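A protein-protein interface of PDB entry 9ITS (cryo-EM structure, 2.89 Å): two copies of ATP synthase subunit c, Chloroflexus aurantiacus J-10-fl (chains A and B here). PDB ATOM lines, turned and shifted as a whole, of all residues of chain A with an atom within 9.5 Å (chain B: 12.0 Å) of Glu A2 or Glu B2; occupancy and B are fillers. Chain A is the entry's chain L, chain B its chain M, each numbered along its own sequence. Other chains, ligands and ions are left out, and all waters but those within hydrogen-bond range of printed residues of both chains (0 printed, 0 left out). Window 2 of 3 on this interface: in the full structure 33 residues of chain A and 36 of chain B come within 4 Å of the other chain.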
ATOM      1  N   MET A   1       5.390 -23.963  19.908  1.00  0.00           N
ATOM      2  CA  MET A   1       6.406 -23.116  20.522  1.00  0.00           C
ATOM      3  C   MET A   1       7.586 -23.951  21.006  1.00  0.00           C
ATOM      4  O   MET A   1       7.423 -25.105  21.401  1.00  0.00           O
ATOM      5  CB  MET A   1       5.811 -22.318  21.683  1.00  0.00           C
ATOM      6  CG  MET A   1       4.662 -21.407  21.286  1.00  0.00           C
ATOM      7  SD  MET A   1       3.923 -20.566  22.698  1.00  0.00           S
ATOM      8  CE  MET A   1       2.512 -19.780  21.923  1.00  0.00           C
ATOM      9  N   GLU A   2       8.781 -23.357  20.971  1.00  0.00           N
ATOM     10  CA  GLU A   2       9.984 -24.073  21.379  1.00  0.00           C
ATOM     11  C   GLU A   2      10.102 -24.198  22.893  1.00  0.00           C
ATOM     12  O   GLU A   2      10.708 -25.156  23.384  1.00  0.00           O
ATOM     13  CB  GLU A   2      11.224 -23.381  20.807  1.00  0.00           C
ATOM     14  CG  GLU A   2      11.358 -21.913  21.187  1.00  0.00           C
ATOM     15  CD  GLU A   2      12.248 -21.701  22.396  1.00  0.00           C
ATOM     16  OE1 GLU A   2      13.023 -22.620  22.733  1.00  0.00           O
ATOM     17  OE2 GLU A   2      12.173 -20.616  23.008  1.00  0.00           O
ATOM     18  N   GLY A   3       9.539 -23.255  23.642  1.00  0.00           N
ATOM     19  CA  GLY A   3       9.651 -23.234  25.085  1.00  0.00           C
ATOM     20  C   GLY A   3       8.560 -23.958  25.843  1.00  0.00           C
ATOM     21  O   GLY A   3       8.504 -23.845  27.072  1.00  0.00           O
ATOM     22  N   LEU A   4       7.688 -24.697  25.155  1.00  0.00           N
ATOM     23  CA  LEU A   4       6.592 -25.387  25.827  1.00  0.00           C
ATOM     24  C   LEU A   4       7.050 -26.580  26.654  1.00  0.00           C
ATOM     25  O   LEU A   4       6.265 -27.076  27.468  1.00  0.00           O
ATOM     26  CB  LEU A   4       5.553 -25.851  24.805  1.00  0.00           C
ATOM     27  CG  LEU A   4       4.673 -24.768  24.182  1.00  0.00           C
ATOM     28  CD1 LEU A   4       3.592 -25.394  23.315  1.00  0.00           C
ATOM     29  CD2 LEU A   4       4.059 -23.887  25.259  1.00  0.00           C
ATOM     30  N   ASN A   5       8.284 -27.054  26.468  1.00  0.00           N
ATOM     31  CA  ASN A   5       8.732 -28.243  27.185  1.00  0.00           C
ATOM     32  C   ASN A   5       8.908 -27.961  28.674  1.00  0.00           C
ATOM     33  O   ASN A   5       8.232 -28.569  29.513  1.00  0.00           O
ATOM     34  CB  ASN A   5      10.030 -28.769  26.569  1.00  0.00           C
ATOM     35  CG  ASN A   5      11.047 -27.671  26.318  1.00  0.00           C
ATOM     36  OD1 ASN A   5      10.724 -26.485  26.384  1.00  0.00           O
ATOM     37  ND2 ASN A   5      12.282 -28.063  26.033  1.00  0.00           N
ATOM     38  N   LEU A   6       9.795 -27.020  29.016  1.00  0.00           N
ATOM     39  CA  LEU A   6      10.110 -26.752  30.417  1.00  0.00           C
ATOM     40  C   LEU A   6       8.875 -26.308  31.187  1.00  0.00           C
ATOM     41  O   LEU A   6       8.642 -26.768  32.313  1.00  0.00           O
ATOM     42  CB  LEU A   6      11.213 -25.696  30.514  1.00  0.00           C
ATOM     43  CG  LEU A   6      12.642 -26.192  30.747  1.00  0.00           C
ATOM     44  CD1 LEU A   6      13.067 -27.170  29.663  1.00  0.00           C
ATOM     45  CD2 LEU A   6      13.609 -25.020  30.819  1.00  0.00           C
ATOM     46  N   VAL A   7       8.062 -25.437  30.582  1.00  0.00           N
ATOM     47  CA  VAL A   7       6.799 -25.031  31.194  1.00  0.00           C
ATOM     48  C   VAL A   7       5.950 -26.253  31.502  1.00  0.00           C
ATOM     49  O   VAL A   7       5.414 -26.390  32.611  1.00  0.00           O
ATOM     50  CB  VAL A   7       6.055 -24.040  30.280  1.00  0.00           C
ATOM     51  CG1 VAL A   7       4.769 -23.571  30.940  1.00  0.00           C
ATOM     52  CG2 VAL A   7       6.949 -22.861  29.937  1.00  0.00           C
ATOM     53  N   ALA A   8       5.855 -27.183  30.546  1.00  0.00           N
ATOM     54  CA  ALA A   8       5.138 -28.427  30.797  1.00  0.00           C
ATOM     55  C   ALA A   8       5.741 -29.167  31.981  1.00  0.00           C
ATOM     56  O   ALA A   8       5.010 -29.617  32.871  1.00  0.00           O
ATOM     57  CB  ALA A   8       5.148 -29.305  29.548  1.00  0.00           C
ATOM     58  N   MET B   1       3.181 -26.184  16.367  1.00  0.00           N
ATOM     59  CA  MET B   1       3.073 -26.058  17.816  1.00  0.00           C
ATOM     60  C   MET B   1       3.614 -27.298  18.519  1.00  0.00           C
ATOM     61  O   MET B   1       2.850 -28.115  19.033  1.00  0.00           O
ATOM     62  CB  MET B   1       1.620 -25.811  18.224  1.00  0.00           C
ATOM     63  CG  MET B   1       1.066 -24.474  17.764  1.00  0.00           C
ATOM     64  SD  MET B   1       1.866 -23.077  18.579  1.00  0.00           S
ATOM     65  CE  MET B   1       1.075 -23.124  20.184  1.00  0.00           C
ATOM     66  N   GLU B   2       4.937 -27.434  18.532  1.00  0.00           N
ATOM     67  CA  GLU B   2       5.569 -28.562  19.195  1.00  0.00           C
ATOM     68  C   GLU B   2       5.498 -28.403  20.712  1.00  0.00           C
ATOM     69  O   GLU B   2       5.386 -27.297  21.248  1.00  0.00           O
ATOM     70  CB  GLU B   2       7.025 -28.701  18.747  1.00  0.00           C
ATOM     71  CG  GLU B   2       7.941 -27.593  19.244  1.00  0.00           C
ATOM     72  CD  GLU B   2       7.991 -26.403  18.305  1.00  0.00           C
ATOM     73  OE1 GLU B   2       7.137 -26.320  17.397  1.00  0.00           O
ATOM     74  OE2 GLU B   2       8.885 -25.548  18.476  1.00  0.00           O
ATOM     75  N   GLY B   3       5.556 -29.536  21.407  1.00  0.00           N
ATOM     76  CA  GLY B   3       5.506 -29.540  22.854  1.00  0.00           C
ATOM     77  C   GLY B   3       4.126 -29.391  23.450  1.00  0.00           C
ATOM     78  O   GLY B   3       4.007 -29.302  24.677  1.00  0.00           O
ATOM     79  N   LEU B   4       3.079 -29.357  22.623  1.00  0.00           N
ATOM     80  CA  LEU B   4       1.723 -29.229  23.146  1.00  0.00           C
ATOM     81  C   LEU B   4       1.277 -30.497  23.863  1.00  0.00           C
ATOM     82  O   LEU B   4       0.535 -30.423  24.852  1.00  0.00           O
ATOM     83  CB  LEU B   4       0.759 -28.886  22.010  1.00  0.00           C
ATOM     84  CG  LEU B   4      -0.425 -27.984  22.360  1.00  0.00           C
ATOM     85  CD1 LEU B   4       0.060 -26.653  22.910  1.00  0.00           C
ATOM     86  CD2 LEU B   4      -1.317 -27.772  21.147  1.00  0.00           C
ATOM     87  N   ASN B   5       1.717 -31.664  23.383  1.00  0.00           N
ATOM     88  CA  ASN B   5       1.390 -32.917  24.054  1.00  0.00           C
ATOM     89  C   ASN B   5       2.006 -32.987  25.444  1.00  0.00           C
ATOM     90  O   ASN B   5       1.399 -33.553  26.361  1.00  0.00           O
ATOM     91  CB  ASN B   5       1.854 -34.101  23.206  1.00  0.00           C
ATOM     92  CG  ASN B   5       3.307 -33.985  22.791  1.00  0.00           C
ATOM     93  OD1 ASN B   5       3.921 -32.927  22.931  1.00  0.00           O
ATOM     94  ND2 ASN B   5       3.865 -35.075  22.279  1.00  0.00           N
ATOM     95  N   LEU B   6       3.206 -32.428  25.619  1.00  0.00           N
ATOM     96  CA  LEU B   6       3.813 -32.375  26.946  1.00  0.00           C
ATOM     97  C   LEU B   6       2.976 -31.529  27.897  1.00  0.00           C
ATOM     98  O   LEU B   6       2.780 -31.898  29.062  1.00  0.00           O
ATOM     99  CB  LEU B   6       5.234 -31.823  26.847  1.00  0.00           C
ATOM    100  CG  LEU B   6       6.188 -32.563  25.909  1.00  0.00           C
ATOM    101  CD1 LEU B   6       7.519 -31.832  25.813  1.00  0.00           C
ATOM    102  CD2 LEU B   6       6.390 -33.996  26.374  1.00  0.00           C
ATOM    103  N   VAL B   7       2.471 -30.392  27.414  1.00  0.00           N
ATOM    104  CA  VAL B   7       1.610 -29.545  28.235  1.00  0.00           C
ATOM    105  C   VAL B   7       0.318 -30.272  28.578  1.00  0.00           C
ATOM    106  O   VAL B   7      -0.188 -30.173  29.702  1.00  0.00           O
ATOM    107  CB  VAL B   7       1.338 -28.209  27.518  1.00  0.00           C
ATOM    108  CG1 VAL B   7       0.505 -27.290  28.397  1.00  0.00           C
ATOM    109  CG2 VAL B   7       2.648 -27.540  27.136  1.00  0.00           C
ATOM    110  N   ALA B   8      -0.236 -31.015  27.615  1.00  0.00           N
ATOM    111  CA  ALA B   8      -1.440 -31.799  27.876  1.00  0.00           C
ATOM    112  C   ALA B   8      -1.194 -32.843  28.959  1.00  0.00           C
ATOM    113  O   ALA B   8      -1.989 -32.986  29.898  1.00  0.00           O
ATOM    114  CB  ALA B   8      -1.914 -32.468  26.587  1.00  0.00           C
ATOM    115  N   THR B   9      -0.086 -33.579  28.842  1.00  0.00           N
ATOM    116  CA  THR B   9       0.266 -34.579  29.843  1.00  0.00           C
ATOM    117  C   THR B   9       0.424 -33.945  31.217  1.00  0.00           C
ATOM    118  O   THR B   9      -0.092 -34.464  32.218  1.00  0.00           O
ATOM    119  CB  THR B   9       1.558 -35.289  29.432  1.00  0.00           C
ATOM    120  OG1 THR B   9       1.520 -35.582  28.029  1.00  0.00           O
ATOM    121  CG2 THR B   9       1.744 -36.576  30.213  1.00  0.00           C
ATOM    122  N   ILE B  70      -1.846 -40.126  25.561  1.00  0.00           N
ATOM    123  CA  ILE B  70      -1.425 -38.911  24.878  1.00  0.00           C
ATOM    124  C   ILE B  70       0.067 -38.926  24.547  1.00  0.00           C
ATOM    125  O   ILE B  70       0.454 -38.562  23.431  1.00  0.00           O
ATOM    126  CB  ILE B  70      -1.800 -37.692  25.738  1.00  0.00           C
ATOM    127  CG1 ILE B  70      -3.295 -37.399  25.606  1.00  0.00           C
ATOM    128  CG2 ILE B  70      -0.962 -36.473  25.376  1.00  0.00           C
ATOM    129  CD1 ILE B  70      -3.879 -36.685  26.791  1.00  0.00           C
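The backbone NH (N) of Glu A2 sits at hydrogen-bond distance from the side-chain carboxylate (OE2) of Glu B2, 3.3 Å away.
The backbone carbonyl oxygen of Glu B2 lies close to the backbone carbonyl oxygen of Met A1, 3.0 Å away.
OD1 of Asn A5 sits close to O of Glu A2 (3.3 Å).
Among the printed residues, pairs that only touch across the chains: Met A1 with Met B1 (3.8 Å), Leu A4 with Glu B2 (3.3 Å), Leu A4 with Gly B3 (3.8 Å), Leu A4 with Leu B4 (3.8 Å), Leu A4 with Val B7 (3.7 Å), Ala A8 with Leu B6 (3.5 Å) and Ala A8 with Val B7 (3.6 Å).
Of chain B, only Glu B2 (3.3 Å) comes within 4 Å of Glu A2.
Printed residues of chain A within 4 Å of Glu B2: Met A1, Glu A2 and Leu A4.
Met A1 touches two residues of chain B.
No residue of chain B comes within 4 Å of Gly A3.
Leu A4 touches four residues of chain B.
No residue of chain B comes within 4 Å of Asn A5.
Of the printed residues of chain A, Gly B3 touches Leu A4.
Of the printed residues of chain A, Leu B6 touches Ala A8 (3.5 Å).
Printed residues of chain A within 4 Å of Val B7: Leu A4 (3.7 Å) and Ala A8 (3.6 Å).
Of the printed residues of chain A, Leu B4 touches Leu A4.
Of the printed residues of chain A, Met B1 touches Met A1 (3.8 Å).
Of the printed residues of chain B, Ala A8 touches Leu B6 (3.5 Å) and Val B7 (3.6 Å).
Asn B5 touches none of the printed residues of chain A.
Thr B9 touches none of the printed residues of chain A.
The nearest residue of chain B that does not touch Glu A2 is Gly B3 (6.8 Å).
The nearest printed residue of chain A that does not touch Val B7 is Val A7 (5.6 Å).
Of the 10 printed residues of chain B, 6 touch a printed residue of chain A.
Hydrophobic or aromatic side chains of chain B that line the printed part of chain A: Met B1, Leu B4, Leu B6 and Val B7.
Of the 8 printed residues of chain A, 4 touch a printed residue of chain B.
Hydrophobic or aromatic side chains of chain A within 4 Å of the printed part of chain B: Leu A4 and Ala A8.
Glu B2 touches its own counterpart, Glu A2.
Leu A4 touches its own counterpart, Leu B4.
Ala A8 touches Leu B6, but with the chains exchanged Leu A6 does not touch Ala B8 (10.9 Å).
Ala A8 touches Val B7, but with the chains exchanged Val A7 does not touch Ala B8 (8.7 Å).
Of the 9 pairs that touch across the chains among the printed residues, 3 have their exchanged pair printed and touching as well.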
